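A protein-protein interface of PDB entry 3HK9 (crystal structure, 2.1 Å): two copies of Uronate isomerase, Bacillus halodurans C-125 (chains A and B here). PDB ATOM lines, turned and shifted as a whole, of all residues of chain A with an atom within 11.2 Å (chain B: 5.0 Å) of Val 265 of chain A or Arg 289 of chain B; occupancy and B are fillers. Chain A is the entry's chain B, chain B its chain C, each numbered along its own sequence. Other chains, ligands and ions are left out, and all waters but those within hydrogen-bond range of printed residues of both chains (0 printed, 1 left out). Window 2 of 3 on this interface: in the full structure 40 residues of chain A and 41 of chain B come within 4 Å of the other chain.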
ATOM      1  N   ALA A  53     -13.750  19.521   1.984  1.00  0.00           N
ATOM      2  CA  ALA A  53     -13.209  20.177   0.800  1.00  0.00           C
ATOM      3  C   ALA A  53     -14.241  21.129   0.199  1.00  0.00           C
ATOM      4  O   ALA A  53     -13.929  22.274  -0.153  1.00  0.00           O
ATOM      5  CB  ALA A  53     -12.803  19.131  -0.235  1.00  0.00           C
ATOM      6  N   ILE A  63      -9.579  27.360   7.417  1.00  0.00           N
ATOM      7  CA  ILE A  63      -9.438  25.935   7.665  1.00  0.00           C
ATOM      8  C   ILE A  63      -8.921  25.685   9.084  1.00  0.00           C
ATOM      9  O   ILE A  63      -9.336  24.731   9.743  1.00  0.00           O
ATOM     10  CB  ILE A  63      -8.478  25.287   6.636  1.00  0.00           C
ATOM     11  CG1 ILE A  63      -8.497  23.764   6.781  1.00  0.00           C
ATOM     12  CG2 ILE A  63      -7.075  25.817   6.824  1.00  0.00           C
ATOM     13  CD1 ILE A  63      -9.834  23.129   6.428  1.00  0.00           C
ATOM     14  N   PRO A 225       0.997   6.273  -6.162  1.00  0.00           N
ATOM     15  CA  PRO A 225       1.011   7.560  -6.856  1.00  0.00           C
ATOM     16  C   PRO A 225       0.993   7.382  -8.376  1.00  0.00           C
ATOM     17  O   PRO A 225       1.248   6.291  -8.888  1.00  0.00           O
ATOM     18  CB  PRO A 225       2.307   8.195  -6.362  1.00  0.00           C
ATOM     19  CG  PRO A 225       3.219   7.005  -6.297  1.00  0.00           C
ATOM     20  CD  PRO A 225       2.336   5.952  -5.635  1.00  0.00           C
ATOM     21  N   PRO A 226       0.699   8.464  -9.115  1.00  0.00           N
ATOM     22  CA  PRO A 226       0.648   8.420 -10.582  1.00  0.00           C
ATOM     23  C   PRO A 226       1.980   7.982 -11.186  1.00  0.00           C
ATOM     24  O   PRO A 226       2.019   7.405 -12.268  1.00  0.00           O
ATOM     25  CB  PRO A 226       0.300   9.862 -10.961  1.00  0.00           C
ATOM     26  CG  PRO A 226      -0.436  10.373  -9.755  1.00  0.00           C
ATOM     27  CD  PRO A 226       0.371   9.813  -8.619  1.00  0.00           C
ATOM     28  N   GLY A 260      -2.932   6.119  -8.578  1.00  0.00           N
ATOM     29  CA  GLY A 260      -3.268   7.461  -9.020  1.00  0.00           C
ATOM     30  C   GLY A 260      -3.356   8.607  -8.028  1.00  0.00           C
ATOM     31  O   GLY A 260      -3.433   9.758  -8.447  1.00  0.00           O
ATOM     32  N   VAL A 261      -3.340   8.326  -6.730  1.00  0.00           N
ATOM     33  CA  VAL A 261      -3.456   9.402  -5.749  1.00  0.00           C
ATOM     34  C   VAL A 261      -2.146  10.144  -5.468  1.00  0.00           C
ATOM     35  O   VAL A 261      -1.085   9.532  -5.364  1.00  0.00           O
ATOM     36  CB  VAL A 261      -4.052   8.869  -4.407  1.00  0.00           C
ATOM     37  CG1 VAL A 261      -3.199   7.737  -3.857  1.00  0.00           C
ATOM     38  CG2 VAL A 261      -4.161  10.001  -3.395  1.00  0.00           C
ATOM     39  N   LYS A 262      -2.228  11.472  -5.383  1.00  0.00           N
ATOM     40  CA  LYS A 262      -1.062  12.298  -5.072  1.00  0.00           C
ATOM     41  C   LYS A 262      -1.362  12.827  -3.672  1.00  0.00           C
ATOM     42  O   LYS A 262      -2.249  13.665  -3.486  1.00  0.00           O
ATOM     43  CB  LYS A 262      -0.911  13.463  -6.061  1.00  0.00           C
ATOM     44  CG  LYS A 262       0.415  14.226  -5.909  1.00  0.00           C
ATOM     45  CD  LYS A 262       0.591  15.318  -6.967  1.00  0.00           C
ATOM     46  CE  LYS A 262       1.937  16.021  -6.823  1.00  0.00           C
ATOM     47  NZ  LYS A 262       2.074  17.208  -7.726  1.00  0.00           N
ATOM     48  N   LYS A 263      -0.625  12.317  -2.692  1.00  0.00           N
ATOM     49  CA  LYS A 263      -0.828  12.676  -1.294  1.00  0.00           C
ATOM     50  C   LYS A 263      -0.485  14.100  -0.875  1.00  0.00           C
ATOM     51  O   LYS A 263       0.460  14.704  -1.364  1.00  0.00           O
ATOM     52  CB  LYS A 263      -0.054  11.703  -0.402  1.00  0.00           C
ATOM     53  CG  LYS A 263      -0.327  10.231  -0.696  1.00  0.00           C
ATOM     54  CD  LYS A 263      -1.775   9.857  -0.408  1.00  0.00           C
ATOM     55  CE  LYS A 263      -2.115  10.028   1.063  1.00  0.00           C
ATOM     56  NZ  LYS A 263      -3.487   9.517   1.355  1.00  0.00           N
ATOM     57  N   ARG A 264      -1.286  14.615   0.051  1.00  0.00           N
ATOM     58  CA  ARG A 264      -1.106  15.937   0.633  1.00  0.00           C
ATOM     59  C   ARG A 264      -0.660  17.096  -0.260  1.00  0.00           C
ATOM     60  O   ARG A 264       0.369  17.715   0.021  1.00  0.00           O
ATOM     61  CB  ARG A 264      -0.129  15.846   1.815  1.00  0.00           C
ATOM     62  CG  ARG A 264      -0.560  14.918   2.952  1.00  0.00           C
ATOM     63  CD  ARG A 264      -0.021  13.502   2.769  1.00  0.00           C
ATOM     64  NE  ARG A 264       1.442  13.462   2.796  1.00  0.00           N
ATOM     65  CZ  ARG A 264       2.169  12.356   2.655  1.00  0.00           C
ATOM     66  NH1 ARG A 264       1.576  11.183   2.478  1.00  0.00           N
ATOM     67  NH2 ARG A 264       3.494  12.424   2.689  1.00  0.00           N
ATOM     68  N   VAL A 265      -1.407  17.407  -1.319  1.00  0.00           N
ATOM     69  CA  VAL A 265      -1.031  18.546  -2.158  1.00  0.00           C
ATOM     70  C   VAL A 265      -1.473  19.812  -1.407  1.00  0.00           C
ATOM     71  O   VAL A 265      -0.996  20.920  -1.671  1.00  0.00           O
ATOM     72  CB  VAL A 265      -1.694  18.495  -3.563  1.00  0.00           C
ATOM     73  CG1 VAL A 265      -1.207  17.263  -4.322  1.00  0.00           C
ATOM     74  CG2 VAL A 265      -3.207  18.486  -3.433  1.00  0.00           C
ATOM     75  N   HIS A 266      -2.393  19.634  -0.464  1.00  0.00           N
ATOM     76  CA  HIS A 266      -2.863  20.738   0.368  1.00  0.00           C
ATOM     77  C   HIS A 266      -2.909  20.210   1.799  1.00  0.00           C
ATOM     78  O   HIS A 266      -3.973  19.866   2.312  1.00  0.00           O
ATOM     79  CB  HIS A 266      -4.247  21.221  -0.070  1.00  0.00           C
ATOM     80  CG  HIS A 266      -4.670  22.495   0.593  1.00  0.00           C
ATOM     81  ND1 HIS A 266      -5.715  23.265   0.130  1.00  0.00           N
ATOM     82  CD2 HIS A 266      -4.184  23.137   1.682  1.00  0.00           C
ATOM     83  CE1 HIS A 266      -5.854  24.327   0.904  1.00  0.00           C
ATOM     84  NE2 HIS A 266      -4.938  24.273   1.853  1.00  0.00           N
ATOM     85  N   PRO A 267      -1.738  20.146   2.459  1.00  0.00           N
ATOM     86  CA  PRO A 267      -1.531  19.667   3.830  1.00  0.00           C
ATOM     87  C   PRO A 267      -2.575  20.051   4.872  1.00  0.00           C
ATOM     88  O   PRO A 267      -3.073  19.191   5.597  1.00  0.00           O
ATOM     89  CB  PRO A 267      -0.146  20.219   4.181  1.00  0.00           C
ATOM     90  CG  PRO A 267       0.559  20.191   2.866  1.00  0.00           C
ATOM     91  CD  PRO A 267      -0.496  20.744   1.930  1.00  0.00           C
ATOM     92  N   ALA A 268      -2.900  21.337   4.948  1.00  0.00           N
ATOM     93  CA  ALA A 268      -3.860  21.829   5.935  1.00  0.00           C
ATOM     94  C   ALA A 268      -5.262  21.219   5.851  1.00  0.00           C
ATOM     95  O   ALA A 268      -6.013  21.264   6.828  1.00  0.00           O
ATOM     96  CB  ALA A 268      -3.951  23.346   5.849  1.00  0.00           C
ATOM     97  N   LEU A 269      -5.621  20.661   4.697  1.00  0.00           N
ATOM     98  CA  LEU A 269      -6.946  20.056   4.528  1.00  0.00           C
ATOM     99  C   LEU A 269      -7.035  18.649   5.098  1.00  0.00           C
ATOM    100  O   LEU A 269      -8.108  18.043   5.103  1.00  0.00           O
ATOM    101  CB  LEU A 269      -7.343  20.021   3.046  1.00  0.00           C
ATOM    102  CG  LEU A 269      -7.754  21.356   2.437  1.00  0.00           C
ATOM    103  CD1 LEU A 269      -8.115  21.171   0.967  1.00  0.00           C
ATOM    104  CD2 LEU A 269      -8.933  21.915   3.222  1.00  0.00           C
ATOM    105  N   GLY A 270      -5.907  18.133   5.576  1.00  0.00           N
ATOM    106  CA  GLY A 270      -5.893  16.793   6.135  1.00  0.00           C
ATOM    107  C   GLY A 270      -6.298  15.762   5.101  1.00  0.00           C
ATOM    108  O   GLY A 270      -5.829  15.804   3.960  1.00  0.00           O
ATOM    109  N   ASP A 271      -7.176  14.841   5.493  1.00  0.00           N
ATOM    110  CA  ASP A 271      -7.640  13.786   4.595  1.00  0.00           C
ATOM    111  C   ASP A 271      -8.284  14.317   3.315  1.00  0.00           C
ATOM    112  O   ASP A 271      -8.391  13.598   2.325  1.00  0.00           O
ATOM    113  CB  ASP A 271      -8.628  12.862   5.318  1.00  0.00           C
ATOM    114  CG  ASP A 271      -7.962  12.030   6.396  1.00  0.00           C
ATOM    115  OD1 ASP A 271      -6.847  11.523   6.149  1.00  0.00           O
ATOM    116  OD2 ASP A 271      -8.555  11.868   7.484  1.00  0.00           O
ATOM    117  N   ALA A 272      -8.698  15.576   3.335  1.00  0.00           N
ATOM    118  CA  ALA A 272      -9.325  16.185   2.165  1.00  0.00           C
ATOM    119  C   ALA A 272      -8.294  16.919   1.301  1.00  0.00           C
ATOM    120  O   ALA A 272      -8.656  17.721   0.432  1.00  0.00           O
ATOM    121  CB  ALA A 272     -10.425  17.156   2.612  1.00  0.00           C
ATOM    122  N   GLY A 273      -7.015  16.630   1.525  1.00  0.00           N
ATOM    123  CA  GLY A 273      -5.975  17.308   0.771  1.00  0.00           C
ATOM    124  C   GLY A 273      -5.236  16.509  -0.287  1.00  0.00           C
ATOM    125  O   GLY A 273      -4.190  16.957  -0.765  1.00  0.00           O
ATOM    126  N   ASP A 274      -5.759  15.343  -0.662  1.00  0.00           N
ATOM    127  CA  ASP A 274      -5.107  14.520  -1.679  1.00  0.00           C
ATOM    128  C   ASP A 274      -5.615  14.865  -3.086  1.00  0.00           C
ATOM    129  O   ASP A 274      -6.772  15.236  -3.269  1.00  0.00           O
ATOM    130  CB  ASP A 274      -5.324  13.028  -1.384  1.00  0.00           C
ATOM    131  CG  ASP A 274      -4.724  12.604  -0.051  1.00  0.00           C
ATOM    132  OD1 ASP A 274      -3.893  13.367   0.489  1.00  0.00           O
ATOM    133  OD2 ASP A 274      -5.072  11.511   0.453  1.00  0.00           O
ATOM    134  N   PHE A 275      -4.734  14.731  -4.072  1.00  0.00           N
ATOM    135  CA  PHE A 275      -5.054  15.053  -5.456  1.00  0.00           C
ATOM    136  C   PHE A 275      -4.948  13.794  -6.319  1.00  0.00           C
ATOM    137  O   PHE A 275      -4.813  12.694  -5.787  1.00  0.00           O
ATOM    138  CB  PHE A 275      -4.098  16.159  -5.937  1.00  0.00           C
ATOM    139  CG  PHE A 275      -4.412  16.708  -7.306  1.00  0.00           C
ATOM    140  CD1 PHE A 275      -5.728  16.943  -7.704  1.00  0.00           C
ATOM    141  CD2 PHE A 275      -3.379  17.040  -8.181  1.00  0.00           C
ATOM    142  CE1 PHE A 275      -6.011  17.507  -8.956  1.00  0.00           C
ATOM    143  CE2 PHE A 275      -3.652  17.603  -9.432  1.00  0.00           C
ATOM    144  CZ  PHE A 275      -4.976  17.838  -9.818  1.00  0.00           C
ATOM    145  N   VAL A 276      -5.013  13.956  -7.639  1.00  0.00           N
ATOM    146  CA  VAL A 276      -4.958  12.826  -8.571  1.00  0.00           C
ATOM    147  C   VAL A 276      -4.062  13.106  -9.772  1.00  0.00           C
ATOM    148  O   VAL A 276      -3.834  14.258 -10.132  1.00  0.00           O
ATOM    149  CB  VAL A 276      -6.386  12.482  -9.105  1.00  0.00           C
ATOM    150  CG1 VAL A 276      -7.004  13.717  -9.763  1.00  0.00           C
ATOM    151  CG2 VAL A 276      -6.325  11.336 -10.127  1.00  0.00           C
ATOM    152  N   GLY A 277      -3.556  12.042 -10.388  1.00  0.00           N
ATOM    153  CA  GLY A 277      -2.718  12.184 -11.568  1.00  0.00           C
ATOM    154  C   GLY A 277      -2.834  10.928 -12.422  1.00  0.00           C
ATOM    155  O   GLY A 277      -3.063   9.843 -11.892  1.00  0.00           O
ATOM    156  N   LEU A 301      -7.439   6.064 -10.123  1.00  0.00           N
ATOM    157  CA  LEU A 301      -8.050   7.346  -9.765  1.00  0.00           C
ATOM    158  C   LEU A 301      -8.321   8.348 -10.886  1.00  0.00           C
ATOM    159  O   LEU A 301      -9.259   9.151 -10.792  1.00  0.00           O
ATOM    160  CB  LEU A 301      -7.200   8.008  -8.670  1.00  0.00           C
ATOM    161  CG  LEU A 301      -7.805   9.148  -7.852  1.00  0.00           C
ATOM    162  CD1 LEU A 301      -9.082   8.669  -7.170  1.00  0.00           C
ATOM    163  CD2 LEU A 301      -6.799   9.618  -6.816  1.00  0.00           C
ATOM    164  N   TRP A 326     -13.158   7.119  -5.443  1.00  0.00           N
ATOM    165  CA  TRP A 326     -12.986   8.515  -5.052  1.00  0.00           C
ATOM    166  C   TRP A 326     -13.543   9.560  -6.025  1.00  0.00           C
ATOM    167  O   TRP A 326     -14.749   9.809  -6.074  1.00  0.00           O
ATOM    168  CB  TRP A 326     -11.479   8.722  -4.880  1.00  0.00           C
ATOM    169  CG  TRP A 326     -11.008   9.681  -3.834  1.00  0.00           C
ATOM    170  CD1 TRP A 326     -11.629  10.817  -3.397  1.00  0.00           C
ATOM    171  CD2 TRP A 326      -9.732   9.643  -3.185  1.00  0.00           C
ATOM    172  NE1 TRP A 326     -10.811  11.494  -2.517  1.00  0.00           N
ATOM    173  CE2 TRP A 326      -9.640  10.794  -2.371  1.00  0.00           C
ATOM    174  CE3 TRP A 326      -8.654   8.746  -3.219  1.00  0.00           C
ATOM    175  CZ2 TRP A 326      -8.508  11.073  -1.594  1.00  0.00           C
ATOM    176  CZ3 TRP A 326      -7.527   9.025  -2.445  1.00  0.00           C
ATOM    177  CH2 TRP A 326      -7.464  10.179  -1.644  1.00  0.00           C
ATOM    178  N   PHE A 327     -12.641  10.177  -6.784  1.00  0.00           N
ATOM    179  CA  PHE A 327     -13.008  11.197  -7.761  1.00  0.00           C
ATOM    180  C   PHE A 327     -13.699  10.592  -8.983  1.00  0.00           C
ATOM    181  O   PHE A 327     -14.161  11.319  -9.866  1.00  0.00           O
ATOM    182  CB  PHE A 327     -11.761  11.997  -8.166  1.00  0.00           C
ATOM    183  CG  PHE A 327     -11.020  12.593  -6.984  1.00  0.00           C
ATOM    184  CD1 PHE A 327     -11.679  13.427  -6.082  1.00  0.00           C
ATOM    185  CD2 PHE A 327      -9.678  12.286  -6.753  1.00  0.00           C
ATOM    186  CE1 PHE A 327     -11.010  13.949  -4.957  1.00  0.00           C
ATOM    187  CE2 PHE A 327      -9.000  12.796  -5.639  1.00  0.00           C
ATOM    188  CZ  PHE A 327      -9.668  13.630  -4.738  1.00  0.00           C
ATOM    189  N   GLU B 285      -1.108  23.726  -9.619  1.00  0.00           N
ATOM    190  CA  GLU B 285      -1.104  23.235  -8.252  1.00  0.00           C
ATOM    191  C   GLU B 285      -0.141  24.070  -7.399  1.00  0.00           C
ATOM    192  O   GLU B 285      -0.497  24.553  -6.324  1.00  0.00           O
ATOM    193  CB  GLU B 285      -0.657  21.772  -8.234  1.00  0.00           C
ATOM    194  CG  GLU B 285      -0.703  21.130  -6.865  1.00  0.00           C
ATOM    195  CD  GLU B 285       0.198  19.915  -6.772  1.00  0.00           C
ATOM    196  OE1 GLU B 285       0.173  19.084  -7.701  1.00  0.00           O
ATOM    197  OE2 GLU B 285       0.929  19.790  -5.764  1.00  0.00           O
ATOM    198  N   HIS B 286       1.087  24.227  -7.881  1.00  0.00           N
ATOM    199  CA  HIS B 286       2.093  24.991  -7.154  1.00  0.00           C
ATOM    200  C   HIS B 286       1.619  26.421  -6.894  1.00  0.00           C
ATOM    201  O   HIS B 286       1.761  26.938  -5.785  1.00  0.00           O
ATOM    202  CB  HIS B 286       3.401  25.022  -7.940  1.00  0.00           C
ATOM    203  CG  HIS B 286       4.500  25.766  -7.249  1.00  0.00           C
ATOM    204  ND1 HIS B 286       5.428  25.145  -6.439  1.00  0.00           N
ATOM    205  CD2 HIS B 286       4.801  27.087  -7.223  1.00  0.00           C
ATOM    206  CE1 HIS B 286       6.253  26.051  -5.945  1.00  0.00           C
ATOM    207  NE2 HIS B 286       5.895  27.238  -6.404  1.00  0.00           N
ATOM    208  N   LEU B 287       1.054  27.056  -7.916  1.00  0.00           N
ATOM    209  CA  LEU B 287       0.569  28.426  -7.777  1.00  0.00           C
ATOM    210  C   LEU B 287      -0.511  28.564  -6.707  1.00  0.00           C
ATOM    211  O   LEU B 287      -0.465  29.474  -5.883  1.00  0.00           O
ATOM    212  CB  LEU B 287       0.029  28.938  -9.114  1.00  0.00           C
ATOM    213  CG  LEU B 287       1.076  29.380 -10.134  1.00  0.00           C
ATOM    214  CD1 LEU B 287       0.412  29.604 -11.494  1.00  0.00           C
ATOM    215  CD2 LEU B 287       1.750  30.659  -9.640  1.00  0.00           C
ATOM    216  N   LEU B 288      -1.480  27.655  -6.716  1.00  0.00           N
ATOM    217  CA  LEU B 288      -2.569  27.702  -5.752  1.00  0.00           C
ATOM    218  C   LEU B 288      -2.084  27.510  -4.316  1.00  0.00           C
ATOM    219  O   LEU B 288      -2.467  28.268  -3.417  1.00  0.00           O
ATOM    220  CB  LEU B 288      -3.618  26.639  -6.098  1.00  0.00           C
ATOM    221  CG  LEU B 288      -4.287  26.795  -7.472  1.00  0.00           C
ATOM    222  CD1 LEU B 288      -5.107  25.550  -7.794  1.00  0.00           C
ATOM    223  CD2 LEU B 288      -5.171  28.045  -7.480  1.00  0.00           C
ATOM    224  N   ARG B 289      -1.242  26.504  -4.103  1.00  0.00           N
ATOM    225  CA  ARG B 289      -0.724  26.218  -2.772  1.00  0.00           C
ATOM    226  C   ARG B 289       0.258  27.256  -2.235  1.00  0.00           C
ATOM    227  O   ARG B 289       0.178  27.641  -1.070  1.00  0.00           O
ATOM    228  CB  ARG B 289      -0.041  24.846  -2.741  1.00  0.00           C
ATOM    229  CG  ARG B 289       0.598  24.519  -1.387  1.00  0.00           C
ATOM    230  CD  ARG B 289       1.270  23.150  -1.360  1.00  0.00           C
ATOM    231  NE  ARG B 289       2.278  23.014  -2.407  1.00  0.00           N
ATOM    232  CZ  ARG B 289       2.130  22.276  -3.503  1.00  0.00           C
ATOM    233  NH1 ARG B 289       1.009  21.591  -3.705  1.00  0.00           N
ATOM    234  NH2 ARG B 289       3.101  22.225  -4.404  1.00  0.00           N
ATOM    235  N   GLU B 290       1.182  27.706  -3.078  1.00  0.00           N
ATOM    236  CA  GLU B 290       2.195  28.664  -2.641  1.00  0.00           C
ATOM    237  C   GLU B 290       1.759  30.122  -2.591  1.00  0.00           C
ATOM    238  O   GLU B 290       2.448  30.955  -2.002  1.00  0.00           O
ATOM    239  CB  GLU B 290       3.443  28.554  -3.524  1.00  0.00           C
ATOM    240  CG  GLU B 290       4.085  27.173  -3.545  1.00  0.00           C
ATOM    241  CD  GLU B 290       4.317  26.606  -2.154  1.00  0.00           C
ATOM    242  OE1 GLU B 290       4.555  27.401  -1.221  1.00  0.00           O
ATOM    243  OE2 GLU B 290       4.276  25.364  -1.997  1.00  0.00           O
ATOM    244  N   TYR B 291       0.627  30.437  -3.207  1.00  0.00           N
ATOM    245  CA  TYR B 291       0.141  31.813  -3.223  1.00  0.00           C
ATOM    246  C   TYR B 291      -1.321  31.868  -2.781  1.00  0.00           C
ATOM    247  O   TYR B 291      -2.204  32.273  -3.543  1.00  0.00           O
ATOM    248  CB  TYR B 291       0.317  32.396  -4.631  1.00  0.00           C
ATOM    249  CG  TYR B 291       1.770  32.519  -5.042  1.00  0.00           C
ATOM    250  CD1 TYR B 291       2.520  33.654  -4.712  1.00  0.00           C
ATOM    251  CD2 TYR B 291       2.409  31.484  -5.720  1.00  0.00           C
ATOM    252  CE1 TYR B 291       3.873  33.751  -5.054  1.00  0.00           C
ATOM    253  CE2 TYR B 291       3.757  31.565  -6.064  1.00  0.00           C
ATOM    254  CZ  TYR B 291       4.482  32.698  -5.733  1.00  0.00           C
ATOM    255  OH  TYR B 291       5.807  32.776  -6.094  1.00  0.00           O
ATOM    256  N   PRO B 292      -1.585  31.475  -1.524  1.00  0.00           N
ATOM    257  CA  PRO B 292      -2.928  31.456  -0.940  1.00  0.00           C
ATOM    258  C   PRO B 292      -3.636  32.804  -0.908  1.00  0.00           C
ATOM    259  O   PRO B 292      -4.863  32.857  -0.773  1.00  0.00           O
ATOM    260  CB  PRO B 292      -2.686  30.890   0.458  1.00  0.00           C
ATOM    261  CG  PRO B 292      -1.320  31.403   0.787  1.00  0.00           C
ATOM    262  CD  PRO B 292      -0.575  31.133  -0.505  1.00  0.00           C
ATOM    263  N   LYS B 315      -9.456  21.002  -4.018  1.00  0.00           N
ATOM    264  CA  LYS B 315      -8.305  21.175  -3.127  1.00  0.00           C
ATOM    265  C   LYS B 315      -8.033  22.610  -2.704  1.00  0.00           C
ATOM    266  O   LYS B 315      -7.544  22.846  -1.600  1.00  0.00           O
ATOM    267  CB  LYS B 315      -7.022  20.658  -3.793  1.00  0.00           C
ATOM    268  CG  LYS B 315      -7.063  19.253  -4.384  1.00  0.00           C
ATOM    269  CD  LYS B 315      -7.265  18.176  -3.336  1.00  0.00           C
ATOM    270  CE  LYS B 315      -8.746  17.930  -3.094  1.00  0.00           C
ATOM    271  NZ  LYS B 315      -8.957  16.748  -2.230  1.00  0.00           N
ATOM    272  N   PHE B 316      -8.331  23.565  -3.582  1.00  0.00           N
ATOM    273  CA  PHE B 316      -8.033  24.963  -3.292  1.00  0.00           C
ATOM    274  C   PHE B 316      -9.180  25.929  -3.525  1.00  0.00           C
ATOM    275  O   PHE B 316      -9.715  26.010  -4.629  1.00  0.00           O
ATOM    276  CB  PHE B 316      -6.832  25.398  -4.132  1.00  0.00           C
ATOM    277  CG  PHE B 316      -5.609  24.553  -3.916  1.00  0.00           C
ATOM    278  CD1 PHE B 316      -4.814  24.732  -2.788  1.00  0.00           C
ATOM    279  CD2 PHE B 316      -5.264  23.562  -4.829  1.00  0.00           C
ATOM    280  CE1 PHE B 316      -3.692  23.936  -2.574  1.00  0.00           C
ATOM    281  CE2 PHE B 316      -4.145  22.760  -4.624  1.00  0.00           C
ATOM    282  CZ  PHE B 316      -3.357  22.947  -3.493  1.00  0.00           C
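No position is printed for both chains.
The side-chain amino group (NZ) of Lys 315 of chain B lies within hydrogen-bond range of the backbone carbonyl oxygen (O) of Ala 272 of chain A.
NZ of Lys 315 of chain B is in hydrogen-bond range of O of Asp 274 of chain A (2.9 Å).
OE1 of Glu 285 of chain B lies within salt-bridge range of NZ of Lys 262 of chain A (2.7 Å).
A ring nitrogen (ND1) of His 266 of chain A lies within hydrogen-bond range of the backbone carbonyl oxygen of Lys 315 of chain B.
O of Val 265 of chain A is in hydrogen-bond range of NH1 of Arg 289 of chain B, 2.9 Å away.
OE2 of Glu 285 of chain B touches CG1 of Val 265 of chain A, 3.6 Å away.
Val 265 of chain A touches Phe 316 of chain B (O to CZ, 3.6 Å).
His 266 of chain A touches Phe 316 of chain B.
Leu 269 of chain A touches Lys 315 of chain B.
Of the printed residues of chain B, Lys 262 of chain A touches Glu 285 (2.7 Å).
Val 265 of chain A touches just these residues of chain B: Glu 285, Arg 289 and Phe 316.
Printed residues of chain B within 4 Å of His 266 of chain A: Lys 315 and Phe 316.
Of the printed residues of chain B, Leu 269 of chain A touches Lys 315 (3.1 Å).
Printed residues of chain B within 4 Å of Asp 274 of chain A: Lys 315 (2.9 Å).
Val 276 of chain A touches none of the printed residues of chain B.
Of chain A, only Lys 262 (2.7 Å) and Val 265 (3.6 Å) come within 4 Å of Glu 285 of chain B.
No residue of chain A comes within 4 Å of His 286 of chain B.
Leu 287 of chain B touches none of the printed residues of chain A.
No residue of chain A comes within 4 Å of Leu 288 of chain B.
Of chain A, only Val 265 comes within 4 Å of Arg 289 of chain B.
Of the printed residues of chain A, Lys 315 of chain B touches His 266, Leu 269, Ala 272 and Asp 274.
Of the printed residues of chain A, Phe 316 of chain B touches Val 265 (3.6 Å) and His 266 (3.4 Å).
The nearest residue of chain B that does not touch Val 265 of chain A is Lys 315 of chain B (4.04 Å).
The nearest printed residue of chain B that does not touch Asp 274 of chain A is Phe 316 of chain B (8.1 Å).
The backbone carbonyl oxygen (O) of Gly 273 of chain A sits at hydrogen-bond distance from the backbone NH (N) of His 266 of chain A, at 3.2 Å.
The backbone NH of Arg 264 of chain A sits at hydrogen-bond distance from the side-chain carboxylate of Asp 274 of chain A (2.9 Å).
N of Val 265 of chain A sits at hydrogen-bond distance from O of Gly 273 of chain A.
The guanidinium group (NE) of Arg 289 of chain B lies within salt-bridge range of the side-chain carboxylate (OE2) of Glu 290 of chain B, 3.1 Å away.
NZ of Lys 263 of chain A is in salt-bridge range of OD2 of Asp 274 of chain A (2.7 Å).
NH1 of Arg 289 of chain B lies within salt-bridge range of OE2 of Glu 285 of chain B (2.7 Å).
Hydrophobic or aromatic side chains of chain B within 4 Å of the printed part of chain A: Phe 316.
Hydrophobic or aromatic side chains of chain A that line the printed part of chain B: Val 265, His 266 and Leu 269.
Among the printed residues, Asp or Glu carboxylates within 4 Å of a Lys or Arg side-chain nitrogen of the other chain: Lys 262 of chain A with Glu 285 of chain B.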
